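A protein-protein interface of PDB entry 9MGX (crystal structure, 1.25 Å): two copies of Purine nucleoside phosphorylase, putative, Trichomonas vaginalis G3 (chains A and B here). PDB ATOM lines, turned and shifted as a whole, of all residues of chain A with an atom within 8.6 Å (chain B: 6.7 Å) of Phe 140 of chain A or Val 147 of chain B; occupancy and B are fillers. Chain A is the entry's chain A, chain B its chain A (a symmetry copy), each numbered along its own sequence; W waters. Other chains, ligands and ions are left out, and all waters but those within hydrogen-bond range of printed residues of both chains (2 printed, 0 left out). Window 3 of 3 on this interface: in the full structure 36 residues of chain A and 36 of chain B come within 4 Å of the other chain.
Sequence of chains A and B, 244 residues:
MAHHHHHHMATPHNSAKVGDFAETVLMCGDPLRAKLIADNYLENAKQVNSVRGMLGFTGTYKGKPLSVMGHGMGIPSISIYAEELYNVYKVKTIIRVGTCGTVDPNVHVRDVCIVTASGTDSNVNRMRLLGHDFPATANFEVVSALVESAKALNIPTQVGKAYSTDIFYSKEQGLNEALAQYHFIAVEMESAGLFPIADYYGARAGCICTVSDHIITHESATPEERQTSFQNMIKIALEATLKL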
ATOM      1  N   ILE A 114     -10.875 -17.514  -8.480  1.00  0.00           N
ATOM      2  CA  ILE A 114      -9.539 -16.948  -8.559  1.00  0.00           C
ATOM      3  C   ILE A 114      -9.703 -15.461  -8.866  1.00  0.00           C
ATOM      4  O   ILE A 114     -10.312 -15.096  -9.876  1.00  0.00           O
ATOM      5  CB  ILE A 114      -8.695 -17.673  -9.618  1.00  0.00           C
ATOM      6  CG1 ILE A 114      -8.459 -19.137  -9.199  1.00  0.00           C
ATOM      7  CG2 ILE A 114      -7.386 -16.932  -9.816  1.00  0.00           C
ATOM      8  CD1 ILE A 114      -7.825 -19.992 -10.286  1.00  0.00           C
ATOM      9  N   VAL A 115      -9.151 -14.615  -8.006  1.00  0.00           N
ATOM     10  CA  VAL A 115      -9.402 -13.176  -8.011  1.00  0.00           C
ATOM     11  C   VAL A 115      -8.383 -12.436  -8.880  1.00  0.00           C
ATOM     12  O   VAL A 115      -7.179 -12.498  -8.632  1.00  0.00           O
ATOM     13  CB  VAL A 115      -9.368 -12.651  -6.567  1.00  0.00           C
ATOM     14  CG1 VAL A 115      -9.540 -11.142  -6.547  1.00  0.00           C
ATOM     15  CG2 VAL A 115     -10.443 -13.318  -5.733  1.00  0.00           C
ATOM     16  N   THR A 116      -8.871 -11.663  -9.859  1.00  0.00           N
ATOM     17  CA  THR A 116      -7.989 -10.831 -10.671  1.00  0.00           C
ATOM     18  C   THR A 116      -7.812  -9.427 -10.093  1.00  0.00           C
ATOM     19  O   THR A 116      -6.738  -8.843 -10.231  1.00  0.00           O
ATOM     20  CB  THR A 116      -8.553 -10.714 -12.081  1.00  0.00           C
ATOM     21  OG1 THR A 116      -9.925 -10.331 -11.984  1.00  0.00           O
ATOM     22  CG2 THR A 116      -8.398 -12.040 -12.812  1.00  0.00           C
ATOM     23  N   THR A 137      -5.113  -5.044  -7.451  1.00  0.00           N
ATOM     24  CA  THR A 137      -4.947  -5.908  -8.614  1.00  0.00           C
ATOM     25  C   THR A 137      -3.999  -7.047  -8.257  1.00  0.00           C
ATOM     26  O   THR A 137      -2.888  -6.804  -7.778  1.00  0.00           O
ATOM     27  CB  THR A 137      -4.401  -5.104  -9.813  1.00  0.00           C
ATOM     28  OG1 THR A 137      -5.217  -3.948 -10.004  1.00  0.00           O
ATOM     29  CG2 THR A 137      -4.405  -5.931 -11.091  1.00  0.00           C
ATOM     30  N   ALA A 138      -4.426  -8.280  -8.513  1.00  0.00           N
ATOM     31  CA  ALA A 138      -3.561  -9.429  -8.309  1.00  0.00           C
ATOM     32  C   ALA A 138      -2.434  -9.444  -9.340  1.00  0.00           C
ATOM     33  O   ALA A 138      -2.579  -8.973 -10.472  1.00  0.00           O
ATOM     34  CB  ALA A 138      -4.366 -10.731  -8.403  1.00  0.00           C
ATOM     35  N   ASN A 139      -1.294 -10.001  -8.942  1.00  0.00           N
ATOM     36  CA  ASN A 139      -0.193 -10.187  -9.875  1.00  0.00           C
ATOM     37  C   ASN A 139      -0.547 -11.244 -10.921  1.00  0.00           C
ATOM     38  O   ASN A 139      -1.055 -12.315 -10.597  1.00  0.00           O
ATOM     39  CB  ASN A 139       1.048 -10.616  -9.094  1.00  0.00           C
ATOM     40  CG  ASN A 139       2.179 -11.036  -9.998  1.00  0.00           C
ATOM     41  OD1 ASN A 139       2.336 -12.217 -10.301  1.00  0.00           O
ATOM     42  ND2 ASN A 139       2.963 -10.082 -10.437  1.00  0.00           N
ATOM     43  N   PHE A 140      -0.220 -10.956 -12.179  1.00  0.00           N
ATOM     44  CA  PHE A 140      -0.626 -11.835 -13.271  1.00  0.00           C
ATOM     45  C   PHE A 140       0.028 -13.210 -13.194  1.00  0.00           C
ATOM     46  O   PHE A 140      -0.613 -14.217 -13.507  1.00  0.00           O
ATOM     47  CB  PHE A 140      -0.312 -11.161 -14.609  1.00  0.00           C
ATOM     48  CG  PHE A 140      -0.533 -12.053 -15.786  1.00  0.00           C
ATOM     49  CD1 PHE A 140      -1.812 -12.281 -16.241  1.00  0.00           C
ATOM     50  CD2 PHE A 140       0.522 -12.712 -16.395  1.00  0.00           C
ATOM     51  CE1 PHE A 140      -2.050 -13.122 -17.315  1.00  0.00           C
ATOM     52  CE2 PHE A 140       0.293 -13.558 -17.482  1.00  0.00           C
ATOM     53  CZ  PHE A 140      -0.993 -13.761 -17.925  1.00  0.00           C
ATOM     54  N   GLU A 141       1.306 -13.273 -12.828  1.00  0.00           N
ATOM     55  CA  GLU A 141       1.953 -14.571 -12.696  1.00  0.00           C
ATOM     56  C   GLU A 141       1.279 -15.410 -11.612  1.00  0.00           C
ATOM     57  O   GLU A 141       1.138 -16.636 -11.765  1.00  0.00           O
ATOM     58  CB  GLU A 141       3.447 -14.389 -12.422  1.00  0.00           C
ATOM     59  CG  GLU A 141       4.274 -13.967 -13.645  1.00  0.00           C
ATOM     60  CD  GLU A 141       4.312 -12.477 -13.892  1.00  0.00           C
ATOM     61  OE1 GLU A 141       3.688 -11.701 -13.143  1.00  0.00           O
ATOM     62  OE2 GLU A 141       5.003 -12.071 -14.850  1.00  0.00           O
ATOM     63  N   VAL A 142       0.844 -14.778 -10.519  1.00  0.00           N
ATOM     64  CA  VAL A 142       0.149 -15.517  -9.468  1.00  0.00           C
ATOM     65  C   VAL A 142      -1.201 -16.017  -9.969  1.00  0.00           C
ATOM     66  O   VAL A 142      -1.553 -17.185  -9.782  1.00  0.00           O
ATOM     67  CB  VAL A 142       0.000 -14.666  -8.194  1.00  0.00           C
ATOM     68  CG1 VAL A 142      -0.816 -15.415  -7.148  1.00  0.00           C
ATOM     69  CG2 VAL A 142       1.361 -14.297  -7.645  1.00  0.00           C
ATOM     70  N   VAL A 143      -1.984 -15.136 -10.604  1.00  0.00           N
ATOM     71  CA  VAL A 143      -3.273 -15.559 -11.140  1.00  0.00           C
ATOM     72  C   VAL A 143      -3.077 -16.733 -12.091  1.00  0.00           C
ATOM     73  O   VAL A 143      -3.788 -17.739 -12.024  1.00  0.00           O
ATOM     74  CB  VAL A 143      -3.973 -14.385 -11.851  1.00  0.00           C
ATOM     75  CG1 VAL A 143      -5.263 -14.853 -12.496  1.00  0.00           C
ATOM     76  CG2 VAL A 143      -4.257 -13.238 -10.905  1.00  0.00           C
ATOM     77  N   SER A 144      -2.115 -16.599 -13.004  1.00  0.00           N
ATOM     78  CA  SER A 144      -1.869 -17.635 -13.999  1.00  0.00           C
ATOM     79  C   SER A 144      -1.453 -18.945 -13.351  1.00  0.00           C
ATOM     80  O   SER A 144      -1.879 -20.021 -13.783  1.00  0.00           O
ATOM     81  CB  SER A 144      -0.774 -17.178 -14.954  1.00  0.00           C
ATOM     82  OG  SER A 144      -1.206 -16.087 -15.739  1.00  0.00           O
ATOM     83  N   ALA A 145      -0.615 -18.875 -12.314  1.00  0.00           N
ATOM     84  CA  ALA A 145      -0.200 -20.097 -11.640  1.00  0.00           C
ATOM     85  C   ALA A 145      -1.394 -20.798 -11.013  1.00  0.00           C
ATOM     86  O   ALA A 145      -1.489 -22.025 -11.057  1.00  0.00           O
ATOM     87  CB  ALA A 145       0.862 -19.787 -10.586  1.00  0.00           C
ATOM     88  N   LEU A 146      -2.309 -20.039 -10.412  1.00  0.00           N
ATOM     89  CA  LEU A 146      -3.515 -20.627  -9.838  1.00  0.00           C
ATOM     90  C   LEU A 146      -4.399 -21.246 -10.920  1.00  0.00           C
ATOM     91  O   LEU A 146      -4.876 -22.378 -10.777  1.00  0.00           O
ATOM     92  CB  LEU A 146      -4.276 -19.565  -9.041  1.00  0.00           C
ATOM     93  CG  LEU A 146      -3.564 -19.097  -7.769  1.00  0.00           C
ATOM     94  CD1 LEU A 146      -4.179 -17.794  -7.288  1.00  0.00           C
ATOM     95  CD2 LEU A 146      -3.647 -20.136  -6.653  1.00  0.00           C
ATOM     96  N   VAL A 147      -4.622 -20.523 -12.022  1.00  0.00           N
ATOM     97  CA  VAL A 147      -5.452 -21.040 -13.108  1.00  0.00           C
ATOM     98  C   VAL A 147      -4.856 -22.323 -13.674  1.00  0.00           C
ATOM     99  O   VAL A 147      -5.562 -23.312 -13.903  1.00  0.00           O
ATOM    100  CB  VAL A 147      -5.644 -19.959 -14.188  1.00  0.00           C
ATOM    101  CG1 VAL A 147      -6.235 -20.573 -15.458  1.00  0.00           C
ATOM    102  CG2 VAL A 147      -6.521 -18.807 -13.662  1.00  0.00           C
ATOM    103  N   GLU A 148      -3.550 -22.322 -13.914  1.00  0.00           N
ATOM    104  CA  GLU A 148      -2.929 -23.483 -14.538  1.00  0.00           C
ATOM    105  C   GLU A 148      -2.874 -24.668 -13.588  1.00  0.00           C
ATOM    106  O   GLU A 148      -3.030 -25.810 -14.023  1.00  0.00           O
ATOM    107  CB  GLU A 148      -1.543 -23.112 -15.055  1.00  0.00           C
ATOM    108  CG  GLU A 148      -1.581 -22.149 -16.226  1.00  0.00           C
ATOM    109  CD  GLU A 148      -2.381 -22.686 -17.407  1.00  0.00           C
ATOM    110  OE1 GLU A 148      -2.125 -23.834 -17.835  1.00  0.00           O
ATOM    111  OE2 GLU A 148      -3.277 -21.964 -17.894  1.00  0.00           O
ATOM    112  N   ALA A 203       6.400  -6.505  -4.754  1.00  0.00           N
ATOM    113  CA  ALA A 203       6.205  -7.922  -4.510  1.00  0.00           C
ATOM    114  C   ALA A 203       4.896  -8.377  -5.159  1.00  0.00           C
ATOM    115  O   ALA A 203       4.262  -7.626  -5.896  1.00  0.00           O
ATOM    116  CB  ALA A 203       6.254  -8.185  -3.009  1.00  0.00           C
ATOM    117  N   ARG A 204       4.508  -9.625  -4.903  1.00  0.00           N
ATOM    118  CA  ARG A 204       3.400 -10.257  -5.596  1.00  0.00           C
ATOM    119  C   ARG A 204       2.360 -10.769  -4.614  1.00  0.00           C
ATOM    120  O   ARG A 204       2.684 -11.227  -3.514  1.00  0.00           O
ATOM    121  CB  ARG A 204       3.897 -11.427  -6.450  1.00  0.00           C
ATOM    122  CG  ARG A 204       4.884 -10.999  -7.512  1.00  0.00           C
ATOM    123  CD  ARG A 204       5.237 -12.149  -8.411  1.00  0.00           C
ATOM    124  NE  ARG A 204       5.729 -13.284  -7.644  1.00  0.00           N
ATOM    125  CZ  ARG A 204       6.221 -14.386  -8.178  1.00  0.00           C
ATOM    126  NH1 ARG A 204       6.304 -14.539  -9.489  1.00  0.00           N
ATOM    127  NH2 ARG A 204       6.646 -15.357  -7.373  1.00  0.00           N
ATOM    128  N   ALA A 205       1.106 -10.725  -5.054  1.00  0.00           N
ATOM    129  CA  ALA A 205      -0.005 -11.255  -4.285  1.00  0.00           C
ATOM    130  C   ALA A 205      -1.093 -11.780  -5.207  1.00  0.00           C
ATOM    131  O   ALA A 205      -1.230 -11.349  -6.361  1.00  0.00           O
ATOM    132  CB  ALA A 205      -0.598 -10.227  -3.323  1.00  0.00           C
ATOM    133  N   GLY A 206      -1.863 -12.727  -4.682  1.00  0.00           N
ATOM    134  CA  GLY A 206      -3.075 -13.191  -5.318  1.00  0.00           C
ATOM    135  C   GLY A 206      -4.050 -13.684  -4.272  1.00  0.00           C
ATOM    136  O   GLY A 206      -3.778 -13.641  -3.068  1.00  0.00           O
ATOM    137  N   LEU A 244       5.969 -20.458  -8.461  1.00  0.00           N
ATOM    138  CA  LEU A 244       6.164 -19.079  -8.029  1.00  0.00           C
ATOM    139  C   LEU A 244       7.422 -18.912  -7.172  1.00  0.00           C
ATOM    140  O   LEU A 244       7.757 -17.776  -6.814  1.00  0.00           O
ATOM    141  CB  LEU A 244       4.934 -18.603  -7.262  1.00  0.00           C
ATOM    142  CG  LEU A 244       3.658 -18.509  -8.103  1.00  0.00           C
ATOM    143  CD1 LEU A 244       2.472 -18.368  -7.172  1.00  0.00           C
ATOM    144  CD2 LEU A 244       3.682 -17.359  -9.118  1.00  0.00           C
ATOM    145  OXT LEU A 244       8.123 -19.878  -6.842  1.00  0.00           O
ATOM    146  N   ILE B 114       0.900  -4.636 -21.323  1.00  0.00           N
ATOM    147  CA  ILE B 114      -0.376  -5.331 -21.318  1.00  0.00           C
ATOM    148  C   ILE B 114      -1.043  -5.028 -19.979  1.00  0.00           C
ATOM    149  O   ILE B 114      -0.474  -5.308 -18.920  1.00  0.00           O
ATOM    150  CB  ILE B 114      -0.183  -6.838 -21.546  1.00  0.00           C
ATOM    151  CG1 ILE B 114       0.381  -7.094 -22.958  1.00  0.00           C
ATOM    152  CG2 ILE B 114      -1.503  -7.555 -21.335  1.00  0.00           C
ATOM    153  CD1 ILE B 114       0.814  -8.534 -23.194  1.00  0.00           C
ATOM    154  N   THR B 116      -3.579  -5.160 -16.871  1.00  0.00           N
ATOM    155  CA  THR B 116      -4.433  -6.051 -16.093  1.00  0.00           C
ATOM    156  C   THR B 116      -5.604  -5.317 -15.439  1.00  0.00           C
ATOM    157  O   THR B 116      -6.681  -5.895 -15.297  1.00  0.00           O
ATOM    158  CB  THR B 116      -3.609  -6.729 -15.007  1.00  0.00           C
ATOM    159  OG1 THR B 116      -2.883  -5.722 -14.302  1.00  0.00           O
ATOM    160  CG2 THR B 116      -2.672  -7.753 -15.631  1.00  0.00           C
ATOM    161  N   PHE B 140      -9.439 -11.874 -18.016  1.00  0.00           N
ATOM    162  CA  PHE B 140      -8.241 -12.700 -17.907  1.00  0.00           C
ATOM    163  C   PHE B 140      -7.914 -13.435 -19.201  1.00  0.00           C
ATOM    164  O   PHE B 140      -6.739 -13.578 -19.551  1.00  0.00           O
ATOM    165  CB  PHE B 140      -8.409 -13.688 -16.750  1.00  0.00           C
ATOM    166  CG  PHE B 140      -7.306 -14.692 -16.667  1.00  0.00           C
ATOM    167  CD1 PHE B 140      -6.089 -14.331 -16.135  1.00  0.00           C
ATOM    168  CD2 PHE B 140      -7.461 -15.971 -17.175  1.00  0.00           C
ATOM    169  CE1 PHE B 140      -5.042 -15.232 -16.066  1.00  0.00           C
ATOM    170  CE2 PHE B 140      -6.412 -16.890 -17.107  1.00  0.00           C
ATOM    171  CZ  PHE B 140      -5.209 -16.507 -16.560  1.00  0.00           C
ATOM    172  N   VAL B 142      -8.487 -12.390 -22.178  1.00  0.00           N
ATOM    173  CA  VAL B 142      -7.906 -11.405 -23.087  1.00  0.00           C
ATOM    174  C   VAL B 142      -6.459 -11.114 -22.706  1.00  0.00           C
ATOM    175  O   VAL B 142      -5.569 -11.104 -23.562  1.00  0.00           O
ATOM    176  CB  VAL B 142      -8.750 -10.120 -23.129  1.00  0.00           C
ATOM    177  CG1 VAL B 142      -8.075  -9.069 -24.000  1.00  0.00           C
ATOM    178  CG2 VAL B 142     -10.143 -10.420 -23.638  1.00  0.00           C
ATOM    179  N   VAL B 143      -6.204 -10.861 -21.416  1.00  0.00           N
ATOM    180  CA  VAL B 143      -4.835 -10.609 -20.980  1.00  0.00           C
ATOM    181  C   VAL B 143      -3.942 -11.777 -21.380  1.00  0.00           C
ATOM    182  O   VAL B 143      -2.849 -11.594 -21.921  1.00  0.00           O
ATOM    183  CB  VAL B 143      -4.788 -10.377 -19.458  1.00  0.00           C
ATOM    184  CG1 VAL B 143      -3.353 -10.219 -18.991  1.00  0.00           C
ATOM    185  CG2 VAL B 143      -5.599  -9.168 -19.045  1.00  0.00           C
ATOM    186  N   SER B 144      -4.400 -12.996 -21.093  1.00  0.00           N
ATOM    187  CA  SER B 144      -3.611 -14.187 -21.382  1.00  0.00           C
ATOM    188  C   SER B 144      -3.350 -14.335 -22.871  1.00  0.00           C
ATOM    189  O   SER B 144      -2.247 -14.715 -23.279  1.00  0.00           O
ATOM    190  CB  SER B 144      -4.345 -15.422 -20.876  1.00  0.00           C
ATOM    191  OG  SER B 144      -4.416 -15.429 -19.466  1.00  0.00           O
ATOM    192  N   ALA B 145      -4.355 -14.045 -23.701  1.00  0.00           N
ATOM    193  CA  ALA B 145      -4.154 -14.149 -25.138  1.00  0.00           C
ATOM    194  C   ALA B 145      -3.089 -13.170 -25.605  1.00  0.00           C
ATOM    195  O   ALA B 145      -2.269 -13.503 -26.461  1.00  0.00           O
ATOM    196  CB  ALA B 145      -5.471 -13.911 -25.876  1.00  0.00           C
ATOM    197  N   LEU B 146      -3.092 -11.952 -25.066  1.00  0.00           N
ATOM    198  CA  LEU B 146      -2.069 -10.972 -25.414  1.00  0.00           C
ATOM    199  C   LEU B 146      -0.685 -11.428 -24.953  1.00  0.00           C
ATOM    200  O   LEU B 146       0.288 -11.365 -25.712  1.00  0.00           O
ATOM    201  CB  LEU B 146      -2.433  -9.611 -24.815  1.00  0.00           C
ATOM    202  CG  LEU B 146      -3.669  -8.955 -25.437  1.00  0.00           C
ATOM    203  CD1 LEU B 146      -4.173  -7.848 -24.529  1.00  0.00           C
ATOM    204  CD2 LEU B 146      -3.371  -8.377 -26.819  1.00  0.00           C
ATOM    205  N   VAL B 147      -0.578 -11.904 -23.708  1.00  0.00           N
ATOM    206  CA  VAL B 147       0.707 -12.366 -23.186  1.00  0.00           C
ATOM    207  C   VAL B 147       1.244 -13.519 -24.025  1.00  0.00           C
ATOM    208  O   VAL B 147       2.425 -13.554 -24.387  1.00  0.00           O
ATOM    209  CB  VAL B 147       0.571 -12.739 -21.698  1.00  0.00           C
ATOM    210  CG1 VAL B 147       1.806 -13.510 -21.227  1.00  0.00           C
ATOM    211  CG2 VAL B 147       0.329 -11.486 -20.837  1.00  0.00           C
ATOM    212  N   GLU B 148       0.384 -14.481 -24.340  1.00  0.00           N
ATOM    213  CA  GLU B 148       0.849 -15.657 -25.063  1.00  0.00           C
ATOM    214  C   GLU B 148       1.192 -15.328 -26.508  1.00  0.00           C
ATOM    215  O   GLU B 148       2.141 -15.891 -27.055  1.00  0.00           O
ATOM    216  CB  GLU B 148      -0.194 -16.766 -24.972  1.00  0.00           C
ATOM    217  CG  GLU B 148      -0.339 -17.335 -23.573  1.00  0.00           C
ATOM    218  CD  GLU B 148       0.969 -17.890 -23.023  1.00  0.00           C
ATOM    219  OE1 GLU B 148       1.622 -18.698 -23.722  1.00  0.00           O
ATOM    220  OE2 GLU B 148       1.350 -17.505 -21.897  1.00  0.00           O
ATOM    221  N   SER B 149       0.454 -14.418 -27.131  1.00  0.00           N
ATOM    222  CA  SER B 149       0.804 -14.008 -28.483  1.00  0.00           C
ATOM    223  C   SER B 149       2.162 -13.317 -28.510  1.00  0.00           C
ATOM    224  O   SER B 149       2.985 -13.594 -29.394  1.00  0.00           O
ATOM    225  CB  SER B 149      -0.286 -13.111 -29.065  1.00  0.00           C
ATOM    226  OG  SER B 149      -1.506 -13.820 -29.194  1.00  0.00           O
ATOM    227  N   ALA B 150       2.430 -12.419 -27.553  1.00  0.00           N
ATOM    228  CA  ALA B 150       3.740 -11.768 -27.511  1.00  0.00           C
ATOM    229  C   ALA B 150       4.861 -12.781 -27.303  1.00  0.00           C
ATOM    230  O   ALA B 150       5.925 -12.674 -27.922  1.00  0.00           O
ATOM    231  CB  ALA B 150       3.757 -10.703 -26.415  1.00  0.00           C
ATOM    232  N   LYS B 151       4.641 -13.773 -26.447  1.00  0.00           N
ATOM    233  CA  LYS B 151       5.652 -14.804 -26.239  1.00  0.00           C
ATOM    234  C   LYS B 151       5.939 -15.566 -27.527  1.00  0.00           C
ATOM    235  O   LYS B 151       7.103 -15.809 -27.874  1.00  0.00           O
ATOM    236  CB  LYS B 151       5.184 -15.763 -25.150  1.00  0.00           C
ATOM    237  CG  LYS B 151       5.362 -15.260 -23.753  1.00  0.00           C
ATOM    238  CD  LYS B 151       4.955 -16.344 -22.768  1.00  0.00           C
ATOM    239  CE  LYS B 151       4.984 -15.849 -21.333  1.00  0.00           C
ATOM    240  NZ  LYS B 151       4.150 -16.702 -20.442  1.00  0.00           N
ATOM    241  N   ALA B 152       4.886 -15.968 -28.246  1.00  0.00           N
ATOM    242  CA  ALA B 152       5.091 -16.711 -29.484  1.00  0.00           C
ATOM    243  C   ALA B 152       5.828 -15.873 -30.519  1.00  0.00           C
ATOM    244  O   ALA B 152       6.575 -16.416 -31.340  1.00  0.00           O
ATOM    245  CB  ALA B 152       3.750 -17.197 -30.037  1.00  0.00           C
ATOM    246  N   ILE B 155       8.364 -11.092 -28.497  1.00  0.00           N
ATOM    247  CA  ILE B 155       8.322  -9.662 -28.196  1.00  0.00           C
ATOM    248  C   ILE B 155       8.177  -9.500 -26.686  1.00  0.00           C
ATOM    249  O   ILE B 155       7.162  -9.927 -26.123  1.00  0.00           O
ATOM    250  CB  ILE B 155       7.170  -8.955 -28.931  1.00  0.00           C
ATOM    251  CG1 ILE B 155       7.321  -9.092 -30.443  1.00  0.00           C
ATOM    252  CG2 ILE B 155       7.113  -7.472 -28.541  1.00  0.00           C
ATOM    253  CD1 ILE B 155       6.102  -8.667 -31.234  1.00  0.00           C
ATOM    254  N   THR B 157       7.227  -8.042 -23.048  1.00  0.00           N
ATOM    255  CA  THR B 157       6.118  -7.230 -22.571  1.00  0.00           C
ATOM    256  C   THR B 157       6.254  -6.942 -21.083  1.00  0.00           C
ATOM    257  O   THR B 157       6.852  -7.708 -20.322  1.00  0.00           O
ATOM    258  CB  THR B 157       4.755  -7.915 -22.772  1.00  0.00           C
ATOM    259  OG1 THR B 157       4.726  -9.146 -22.033  1.00  0.00           O
ATOM    260  CG2 THR B 157       4.498  -8.196 -24.245  1.00  0.00           C
ATOM    261  N   VAL B 159       3.604  -6.381 -17.904  1.00  0.00           N
ATOM    262  CA  VAL B 159       2.221  -6.713 -17.572  1.00  0.00           C
ATOM    263  C   VAL B 159       1.901  -6.048 -16.239  1.00  0.00           C
ATOM    264  O   VAL B 159       2.661  -6.201 -15.279  1.00  0.00           O
ATOM    265  CB  VAL B 159       2.024  -8.240 -17.509  1.00  0.00           C
ATOM    266  CG1 VAL B 159       0.590  -8.564 -17.183  1.00  0.00           C
ATOM    267  CG2 VAL B 159       2.431  -8.897 -18.830  1.00  0.00           C
ATOM    268  N   GLY B 160       0.804  -5.297 -16.165  1.00  0.00           N
ATOM    269  CA  GLY B 160       0.474  -4.647 -14.908  1.00  0.00           C
ATOM    270  C   GLY B 160      -0.555  -3.536 -15.070  1.00  0.00           C
ATOM    271  O   GLY B 160      -1.281  -3.470 -16.061  1.00  0.00           O
ATOM    272  N   ILE B 236       0.872  -8.304 -32.000  1.00  0.00           N
ATOM    273  CA  ILE B 236       0.456  -9.017 -30.795  1.00  0.00           C
ATOM    274  C   ILE B 236      -1.062  -9.014 -30.672  1.00  0.00           C
ATOM    275  O   ILE B 236      -1.689 -10.046 -30.412  1.00  0.00           O
ATOM    276  CB  ILE B 236       1.109  -8.397 -29.547  1.00  0.00           C
ATOM    277  CG1 ILE B 236       2.624  -8.581 -29.544  1.00  0.00           C
ATOM    278  CG2 ILE B 236       0.498  -8.995 -28.268  1.00  0.00           C
ATOM    279  CD1 ILE B 236       3.329  -7.662 -28.539  1.00  0.00           C
ATOM    280  N   ALA B 240      -3.602 -12.176 -30.995  1.00  0.00           N
ATOM    281  CA  ALA B 240      -4.424 -12.507 -29.837  1.00  0.00           C
ATOM    282  C   ALA B 240      -5.881 -12.695 -30.225  1.00  0.00           C
ATOM    283  O   ALA B 240      -6.574 -13.534 -29.637  1.00  0.00           O
ATOM    284  CB  ALA B 240      -4.304 -11.422 -28.767  1.00  0.00           C
HETATM  285  O   HOH W   1      -2.374 -16.700 -18.146  1.00  0.00           O
HETATM  286  O   HOH W   2      -1.360  -7.194 -12.467  1.00  0.00           O
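Phe 140 of chain B touches its own counterpart, Phe 140 of chain A.
Phe 140 of chain A touches Val 143 of chain B, and with the chains exchanged Val 143 of chain A touches Phe 140 of chain B.
Phe 140 of chain A touches Ser 144 of chain B, and with the chains exchanged Ser 144 of chain A touches Phe 140 of chain B.
Phe 140 of chain A touches Val 147 of chain B, and with the chains exchanged Val 147 of chain A touches Phe 140 of chain B.
10 positions are printed for both chains.
Water W1 bridges the side-chain hydroxyl of Ser 144 of chain B (2.7 Å) and the side-chain hydroxyl of Ser 144 of chain A (2.7 Å).
Water W2 lies within hydrogen-bond range of OG1 of Thr 116 of chain B and O of Ala 138 of chain A.
The side-chain hydroxyl (OG) of Ser 144 of chain A sits at hydrogen-bond distance from the backbone carbonyl oxygen (O) of Phe 140 of chain A (3.0 Å).
The backbone NH (N) of Thr 116 of chain B lies within hydrogen-bond range of the backbone carbonyl oxygen (O) of Gly 160 of chain B (3.0 Å).
The side-chain hydroxyl (OG) of Ser 144 of chain B sits at hydrogen-bond distance from the backbone carbonyl oxygen (O) of Phe 140 of chain B (3.0 Å).
Glu 141 of chain A touches none of the printed residues of chain B.
Printed residues of chain B within 4 Å of Val 147 of chain A: Phe 140 (3.9 Å).
Of the printed residues of chain A, Thr 116 of chain B touches Thr 137 (3.6 Å).
Printed residues of chain A within 4 Å of Ser 144 of chain B: Phe 140 (3.9 Å).
Of chain A, only Phe 140 (3.9 Å) comes within 4 Å of Val 147 of chain B.
The nearest printed residue of chain B that does not touch Phe 140 of chain A is Thr 116 of chain B (4.3 Å).
The nearest printed residue of chain A that does not touch Ser 144 of chain B is Ser 144 of chain A (5.0 Å).
Among the printed residues, merely in contact across the chains: Thr 137 of chain A with Thr 116 of chain B (3.6 Å), Phe 140 of chain A with Phe 140 of chain B (3.9 Å), Phe 140 of chain A with Val 143 of chain B (3.6 Å), Phe 140 of chain A with Ser 144 of chain B (3.9 Å), Phe 140 of chain A with Val 147 of chain B (3.9 Å), Phe 140 of chain A with Val 159 of chain B (3.8 Å), Val 143 of chain A with Phe 140 of chain B (3.6 Å), Ser 144 of chain A with Phe 140 of chain B (3.9 Å) and Val 147 of chain A with Phe 140 of chain B (3.9 Å).
Of the 20 printed residues of chain A, 5 touch a printed residue of chain B.
Hydrophobic or aromatic side chains of chain A that line the printed part of chain B: Phe 140, Val 143 and Val 147.
Printed residues of chain B that touch a printed residue of chain A: Thr 116, Phe 140, Val 143, Ser 144, Val 147 and Val 159.
Hydrophobic or aromatic side chains of chain B that line the printed part of chain A: Phe 140, Val 143, Val 147 and Val 159.
Among the printed residues, no Asp or Glu carboxylate lies within 4 Å of a Lys or Arg side-chain nitrogen of the other chain.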
